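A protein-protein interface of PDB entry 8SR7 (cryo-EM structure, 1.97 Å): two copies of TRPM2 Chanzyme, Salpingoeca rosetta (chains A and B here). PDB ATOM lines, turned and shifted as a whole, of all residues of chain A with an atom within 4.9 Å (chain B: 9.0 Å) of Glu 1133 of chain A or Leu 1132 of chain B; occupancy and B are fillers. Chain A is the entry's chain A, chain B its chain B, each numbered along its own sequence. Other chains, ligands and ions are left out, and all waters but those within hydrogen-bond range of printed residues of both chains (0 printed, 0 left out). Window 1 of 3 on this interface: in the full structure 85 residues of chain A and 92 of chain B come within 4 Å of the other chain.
The backbone carbonyl oxygen (O) of Glu 1130 of chain B lies within hydrogen-bond range of the guanidinium group (NH1) of Arg 1135 of chain B (3.4 Å).
OG1 of Thr 1139 of chain B is in hydrogen-bond range of O of Arg 1135 of chain B (2.6 Å).
Among the printed residues, pairs that only touch across the chains: Glu 1133 of chain A with Leu 1132 of chain B (3.4 Å), Lys 1137 of chain A with Arg 1135 of chain B (3.5 Å), Val 1136 of chain A with Arg 1135 of chain B (3.8 Å), Leu 1132 of chain A with Leu 1132 of chain B (3.8 Å) and Val 1136 of chain A with Val 1136 of chain B (3.8 Å).
Printed residues of chain B within 4 Å of Leu 1132 of chain A: Leu 1132.
Printed residues of chain B within 4 Å of Glu 1133 of chain A: Leu 1132 (3.4 Å).
No residue of chain B comes within 4 Å of Ala 1134 of chain A.
Of the printed residues of chain B, Val 1136 of chain A touches Arg 1135 (3.8 Å) and Val 1136 (3.8 Å).
Of the printed residues of chain B, Lys 1137 of chain A touches Arg 1135.
Printed residues of chain A within 4 Å of Leu 1132 of chain B: Leu 1132 (3.8 Å) and Glu 1133 (3.4 Å).
Printed residues of chain A within 4 Å of Arg 1135 of chain B: Val 1136 and Lys 1137.
Printed residues of chain A within 4 Å of Val 1136 of chain B: Val 1136 (3.8 Å).
The nearest residue of chain B that does not touch Glu 1133 of chain A is Glu 1130 of chain B (4.2 Å).
The nearest printed residue of chain B that does not touch Val 1136 of chain A is Leu 1132 of chain B (4.1 Å).
Of the 7 printed residues of chain A, 4 touch a printed residue of chain B.
Hydrophobic or aromatic side chains of chain A that line the printed part of chain B: Leu 1132 and Val 1136.
Among the printed residues, no Asp or Glu carboxylate lies within 4 Å of a Lys or Arg side-chain nitrogen of the other chain.
Leu 1132 of chain B touches its own counterpart, Leu 1132 of chain A.
Val 1136 of chain A touches Arg 1135 of chain B, but with the chains exchanged Arg 1135 of chain A does not touch Val 1136 of chain B (8.0 Å).
Val 1136 of chain B touches its own counterpart, Val 1136 of chain A.
Lys 1137 of chain A touches Arg 1135 of chain B, but with the chains exchanged Arg 1135 of chain A does not touch Lys 1137 of chain B (11.5 Å).
Positions printed for both chains: 1131, 1132, 1133, 1134, 1135, 1136 and 1137.
Of the 5 pairs that touch across the chains among the printed residues, 2 have their exchanged pair printed and touching as well.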
ATOM      1  N   MET A1131     -13.022 -13.973 -25.526  1.00  0.00           N
ATOM      2  CA  MET A1131     -13.313 -14.504 -24.196  1.00  0.00           C
ATOM      3  C   MET A1131     -13.721 -13.385 -23.239  1.00  0.00           C
ATOM      4  O   MET A1131     -13.381 -12.213 -23.443  1.00  0.00           O
ATOM      5  CB  MET A1131     -12.115 -15.276 -23.644  1.00  0.00           C
ATOM      6  CG  MET A1131     -11.728 -16.574 -24.378  1.00  0.00           C
ATOM      7  SD  MET A1131     -12.994 -17.883 -24.367  1.00  0.00           S
ATOM      8  CE  MET A1131     -13.743 -17.835 -25.999  1.00  0.00           C
ATOM      9  N   LEU A1132     -14.525 -13.771 -22.236  1.00  0.00           N
ATOM     10  CA  LEU A1132     -15.061 -12.852 -21.228  1.00  0.00           C
ATOM     11  C   LEU A1132     -13.990 -12.217 -20.342  1.00  0.00           C
ATOM     12  O   LEU A1132     -14.090 -11.019 -20.035  1.00  0.00           O
ATOM     13  CB  LEU A1132     -16.083 -13.590 -20.371  1.00  0.00           C
ATOM     14  CG  LEU A1132     -17.035 -12.733 -19.546  1.00  0.00           C
ATOM     15  CD1 LEU A1132     -18.184 -12.218 -20.383  1.00  0.00           C
ATOM     16  CD2 LEU A1132     -17.547 -13.583 -18.419  1.00  0.00           C
ATOM     17  N   GLU A1133     -12.996 -13.019 -19.904  1.00  0.00           N
ATOM     18  CA  GLU A1133     -11.882 -12.577 -19.051  1.00  0.00           C
ATOM     19  C   GLU A1133     -11.009 -11.522 -19.727  1.00  0.00           C
ATOM     20  O   GLU A1133     -10.636 -10.517 -19.100  1.00  0.00           O
ATOM     21  CB  GLU A1133     -11.028 -13.786 -18.663  1.00  0.00           C
ATOM     22  CG  GLU A1133     -11.766 -14.881 -17.913  1.00  0.00           C
ATOM     23  CD  GLU A1133     -11.723 -14.692 -16.412  1.00  0.00           C
ATOM     24  OE1 GLU A1133     -10.751 -14.084 -15.916  1.00  0.00           O
ATOM     25  OE2 GLU A1133     -12.658 -15.154 -15.726  1.00  0.00           O
ATOM     26  N   ALA A1134     -10.667 -11.769 -21.005  1.00  0.00           N
ATOM     27  CA  ALA A1134      -9.853 -10.868 -21.823  1.00  0.00           C
ATOM     28  C   ALA A1134     -10.569  -9.551 -22.097  1.00  0.00           C
ATOM     29  O   ALA A1134      -9.931  -8.492 -22.108  1.00  0.00           O
ATOM     30  CB  ALA A1134      -9.475 -11.549 -23.133  1.00  0.00           C
ATOM     31  N   ARG A1135     -11.882  -9.622 -22.377  1.00  0.00           N
ATOM     32  CA  ARG A1135     -12.708  -8.442 -22.638  1.00  0.00           C
ATOM     33  C   ARG A1135     -12.871  -7.567 -21.395  1.00  0.00           C
ATOM     34  O   ARG A1135     -12.859  -6.332 -21.510  1.00  0.00           O
ATOM     35  CB  ARG A1135     -14.065  -8.872 -23.179  1.00  0.00           C
ATOM     36  CG  ARG A1135     -14.135  -8.945 -24.683  1.00  0.00           C
ATOM     37  CD  ARG A1135     -15.412  -9.616 -25.130  1.00  0.00           C
ATOM     38  NE  ARG A1135     -15.448  -9.783 -26.576  1.00  0.00           N
ATOM     39  CZ  ARG A1135     -16.383 -10.459 -27.227  1.00  0.00           C
ATOM     40  NH1 ARG A1135     -17.387 -11.039 -26.590  1.00  0.00           N
ATOM     41  NH2 ARG A1135     -16.309 -10.557 -28.550  1.00  0.00           N
ATOM     42  N   VAL A1136     -13.055  -8.201 -20.216  1.00  0.00           N
ATOM     43  CA  VAL A1136     -13.153  -7.499 -18.925  1.00  0.00           C
ATOM     44  C   VAL A1136     -11.819  -6.820 -18.577  1.00  0.00           C
ATOM     45  O   VAL A1136     -11.802  -5.645 -18.154  1.00  0.00           O
ATOM     46  CB  VAL A1136     -13.673  -8.475 -17.842  1.00  0.00           C
ATOM     47  CG1 VAL A1136     -13.458  -8.001 -16.437  1.00  0.00           C
ATOM     48  CG2 VAL A1136     -15.182  -8.590 -17.971  1.00  0.00           C
ATOM     49  N   LYS A1137     -10.693  -7.545 -18.803  1.00  0.00           N
ATOM     50  CA  LYS A1137      -9.321  -7.040 -18.623  1.00  0.00           C
ATOM     51  C   LYS A1137      -9.003  -5.864 -19.547  1.00  0.00           C
ATOM     52  O   LYS A1137      -8.393  -4.873 -19.109  1.00  0.00           O
ATOM     53  CB  LYS A1137      -8.321  -8.161 -18.894  1.00  0.00           C
ATOM     54  CG  LYS A1137      -6.920  -7.884 -18.393  1.00  0.00           C
ATOM     55  CD  LYS A1137      -6.082  -9.144 -18.385  1.00  0.00           C
ATOM     56  CE  LYS A1137      -4.676  -8.864 -18.882  1.00  0.00           C
ATOM     57  NZ  LYS A1137      -4.128  -7.606 -18.306  1.00  0.00           N
ATOM     58  N   GLU B1127      -3.254 -12.781  -7.609  1.00  0.00           N
ATOM     59  CA  GLU B1127      -4.263 -13.766  -8.023  1.00  0.00           C
ATOM     60  C   GLU B1127      -5.675 -13.274  -7.733  1.00  0.00           C
ATOM     61  O   GLU B1127      -6.599 -13.574  -8.499  1.00  0.00           O
ATOM     62  CB  GLU B1127      -4.028 -15.132  -7.377  1.00  0.00           C
ATOM     63  CG  GLU B1127      -2.924 -15.959  -8.024  1.00  0.00           C
ATOM     64  CD  GLU B1127      -2.830 -17.356  -7.449  1.00  0.00           C
ATOM     65  OE1 GLU B1127      -3.448 -17.609  -6.393  1.00  0.00           O
ATOM     66  OE2 GLU B1127      -2.133 -18.202  -8.049  1.00  0.00           O
ATOM     67  N   ARG B1128      -5.873 -12.626  -6.570  1.00  0.00           N
ATOM     68  CA  ARG B1128      -7.194 -12.104  -6.236  1.00  0.00           C
ATOM     69  C   ARG B1128      -7.525 -10.888  -7.113  1.00  0.00           C
ATOM     70  O   ARG B1128      -8.688 -10.704  -7.488  1.00  0.00           O
ATOM     71  CB  ARG B1128      -7.238 -11.772  -4.739  1.00  0.00           C
ATOM     72  CG  ARG B1128      -8.569 -11.283  -4.181  1.00  0.00           C
ATOM     73  CD  ARG B1128      -8.471 -11.004  -2.681  1.00  0.00           C
ATOM     74  NE  ARG B1128      -7.535  -9.932  -2.355  1.00  0.00           N
ATOM     75  CZ  ARG B1128      -7.810  -8.634  -2.387  1.00  0.00           C
ATOM     76  NH1 ARG B1128      -9.006  -8.183  -2.734  1.00  0.00           N
ATOM     77  NH2 ARG B1128      -6.859  -7.763  -2.065  1.00  0.00           N
ATOM     78  N   GLN B1129      -6.510 -10.094  -7.516  1.00  0.00           N
ATOM     79  CA  GLN B1129      -6.765  -8.999  -8.459  1.00  0.00           C
ATOM     80  C   GLN B1129      -6.976  -9.472  -9.901  1.00  0.00           C
ATOM     81  O   GLN B1129      -7.490  -8.691 -10.709  1.00  0.00           O
ATOM     82  CB  GLN B1129      -5.684  -7.913  -8.431  1.00  0.00           C
ATOM     83  CG  GLN B1129      -5.608  -7.126  -7.134  1.00  0.00           C
ATOM     84  CD  GLN B1129      -6.882  -6.356  -6.850  1.00  0.00           C
ATOM     85  OE1 GLN B1129      -7.635  -6.695  -5.938  1.00  0.00           O
ATOM     86  NE2 GLN B1129      -7.130  -5.311  -7.632  1.00  0.00           N
ATOM     87  N   GLU B1130      -6.607 -10.712 -10.253  1.00  0.00           N
ATOM     88  CA  GLU B1130      -6.863 -11.174 -11.619  1.00  0.00           C
ATOM     89  C   GLU B1130      -8.191 -11.906 -11.763  1.00  0.00           C
ATOM     90  O   GLU B1130      -8.483 -12.396 -12.860  1.00  0.00           O
ATOM     91  CB  GLU B1130      -5.742 -12.073 -12.165  1.00  0.00           C
ATOM     92  CG  GLU B1130      -4.391 -11.412 -12.350  1.00  0.00           C
ATOM     93  CD  GLU B1130      -3.291 -12.410 -12.648  1.00  0.00           C
ATOM     94  OE1 GLU B1130      -3.498 -13.616 -12.398  1.00  0.00           O
ATOM     95  OE2 GLU B1130      -2.220 -11.990 -13.132  1.00  0.00           O
ATOM     96  N   MET B1131      -8.956 -12.051 -10.678  1.00  0.00           N
ATOM     97  CA  MET B1131     -10.288 -12.648 -10.736  1.00  0.00           C
ATOM     98  C   MET B1131     -11.267 -11.729 -11.465  1.00  0.00           C
ATOM     99  O   MET B1131     -11.065 -10.511 -11.541  1.00  0.00           O
ATOM    100  CB  MET B1131     -10.799 -12.976  -9.333  1.00  0.00           C
ATOM    101  CG  MET B1131     -10.041 -14.071  -8.557  1.00  0.00           C
ATOM    102  SD  MET B1131     -10.075 -15.728  -9.314  1.00  0.00           S
ATOM    103  CE  MET B1131      -8.465 -15.932 -10.083  1.00  0.00           C
ATOM    104  N   LEU B1132     -12.288 -12.361 -12.065  1.00  0.00           N
ATOM    105  CA  LEU B1132     -13.319 -11.673 -12.846  1.00  0.00           C
ATOM    106  C   LEU B1132     -14.181 -10.718 -12.022  1.00  0.00           C
ATOM    107  O   LEU B1132     -14.503  -9.622 -12.507  1.00  0.00           O
ATOM    108  CB  LEU B1132     -14.197 -12.710 -13.538  1.00  0.00           C
ATOM    109  CG  LEU B1132     -15.057 -12.221 -14.696  1.00  0.00           C
ATOM    110  CD1 LEU B1132     -14.258 -12.118 -15.975  1.00  0.00           C
ATOM    111  CD2 LEU B1132     -16.189 -13.193 -14.863  1.00  0.00           C
ATOM    112  N   GLU B1133     -14.584 -11.143 -10.805  1.00  0.00           N
ATOM    113  CA  GLU B1133     -15.410 -10.354  -9.878  1.00  0.00           C
ATOM    114  C   GLU B1133     -14.720  -9.068  -9.427  1.00  0.00           C
ATOM    115  O   GLU B1133     -15.347  -7.997  -9.392  1.00  0.00           O
ATOM    116  CB  GLU B1133     -15.762 -11.209  -8.659  1.00  0.00           C
ATOM    117  CG  GLU B1133     -16.522 -12.487  -8.967  1.00  0.00           C
ATOM    118  CD  GLU B1133     -18.022 -12.295  -8.945  1.00  0.00           C
ATOM    119  OE1 GLU B1133     -18.497 -11.398  -8.217  1.00  0.00           O
ATOM    120  OE2 GLU B1133     -18.729 -13.043  -9.652  1.00  0.00           O
ATOM    121  N   ALA B1134     -13.431  -9.187  -9.060  1.00  0.00           N
ATOM    122  CA  ALA B1134     -12.599  -8.067  -8.618  1.00  0.00           C
ATOM    123  C   ALA B1134     -12.359  -7.063  -9.739  1.00  0.00           C
ATOM    124  O   ALA B1134     -12.341  -5.853  -9.492  1.00  0.00           O
ATOM    125  CB  ALA B1134     -11.273  -8.582  -8.073  1.00  0.00           C
ATOM    126  N   ARG B1135     -12.114  -7.568 -10.961  1.00  0.00           N
ATOM    127  CA  ARG B1135     -11.889  -6.731 -12.141  1.00  0.00           C
ATOM    128  C   ARG B1135     -13.144  -5.961 -12.549  1.00  0.00           C
ATOM    129  O   ARG B1135     -13.040  -4.792 -12.953  1.00  0.00           O
ATOM    130  CB  ARG B1135     -11.381  -7.589 -13.292  1.00  0.00           C
ATOM    131  CG  ARG B1135      -9.879  -7.681 -13.378  1.00  0.00           C
ATOM    132  CD  ARG B1135      -9.461  -8.740 -14.371  1.00  0.00           C
ATOM    133  NE  ARG B1135      -8.014  -8.910 -14.391  1.00  0.00           N
ATOM    134  CZ  ARG B1135      -7.384  -9.859 -15.067  1.00  0.00           C
ATOM    135  NH1 ARG B1135      -8.043 -10.740 -15.800  1.00  0.00           N
ATOM    136  NH2 ARG B1135      -6.059  -9.927 -15.003  1.00  0.00           N
ATOM    137  N   VAL B1136     -14.321  -6.620 -12.477  1.00  0.00           N
ATOM    138  CA  VAL B1136     -15.621  -5.991 -12.765  1.00  0.00           C
ATOM    139  C   VAL B1136     -15.938  -4.906 -11.725  1.00  0.00           C
ATOM    140  O   VAL B1136     -16.373  -3.792 -12.088  1.00  0.00           O
ATOM    141  CB  VAL B1136     -16.709  -7.085 -12.898  1.00  0.00           C
ATOM    142  CG1 VAL B1136     -18.112  -6.566 -12.811  1.00  0.00           C
ATOM    143  CG2 VAL B1136     -16.621  -7.697 -14.285  1.00  0.00           C
ATOM    144  N   LYS B1137     -15.674  -5.214 -10.428  1.00  0.00           N
ATOM    145  CA  LYS B1137     -15.821  -4.280  -9.298  1.00  0.00           C
ATOM    146  C   LYS B1137     -14.900  -3.065  -9.418  1.00  0.00           C
ATOM    147  O   LYS B1137     -15.331  -1.927  -9.161  1.00  0.00           O
ATOM    148  CB  LYS B1137     -15.511  -5.003  -7.990  1.00  0.00           C
ATOM    149  CG  LYS B1137     -15.976  -4.275  -6.748  1.00  0.00           C
ATOM    150  CD  LYS B1137     -15.949  -5.184  -5.538  1.00  0.00           C
ATOM    151  CE  LYS B1137     -15.415  -4.450  -4.320  1.00  0.00           C
ATOM    152  NZ  LYS B1137     -15.988  -3.082  -4.207  1.00  0.00           N
ATOM    153  N   MET B1138     -13.632  -3.321  -9.798  1.00  0.00           N
ATOM    154  CA  MET B1138     -12.604  -2.302 -10.005  1.00  0.00           C
ATOM    155  C   MET B1138     -12.966  -1.378 -11.161  1.00  0.00           C
ATOM    156  O   MET B1138     -12.826  -0.155 -11.032  1.00  0.00           O
ATOM    157  CB  MET B1138     -11.255  -2.982 -10.252  1.00  0.00           C
ATOM    158  CG  MET B1138     -10.083  -2.042 -10.504  1.00  0.00           C
ATOM    159  SD  MET B1138      -8.568  -2.902 -10.957  1.00  0.00           S
ATOM    160  CE  MET B1138      -7.607  -1.550 -11.631  1.00  0.00           C
ATOM    161  N   THR B1139     -13.499  -1.968 -12.256  1.00  0.00           N
ATOM    162  CA  THR B1139     -13.967  -1.259 -13.453  1.00  0.00           C
ATOM    163  C   THR B1139     -15.148  -0.337 -13.132  1.00  0.00           C
ATOM    164  O   THR B1139     -15.172   0.818 -13.587  1.00  0.00           O
ATOM    165  CB  THR B1139     -14.320  -2.305 -14.526  1.00  0.00           C
ATOM    166  OG1 THR B1139     -13.135  -3.019 -14.887  1.00  0.00           O
ATOM    167  CG2 THR B1139     -14.893  -1.695 -15.806  1.00  0.00           C
ATOM    168  N   ASN B1140     -16.085  -0.834 -12.290  1.00  0.00           N
ATOM    169  CA  ASN B1140     -17.271  -0.095 -11.831  1.00  0.00           C
ATOM    170  C   ASN B1140     -16.893   1.134 -10.988  1.00  0.00           C
ATOM    171  O   ASN B1140     -17.429   2.234 -11.223  1.00  0.00           O
ATOM    172  CB  ASN B1140     -18.177  -1.046 -11.040  1.00  0.00           C
ATOM    173  CG  ASN B1140     -19.638  -0.595 -10.984  1.00  0.00           C
ATOM    174  OD1 ASN B1140     -19.995   0.519 -11.372  1.00  0.00           O
ATOM    175  ND2 ASN B1140     -20.493  -1.481 -10.491  1.00  0.00           N
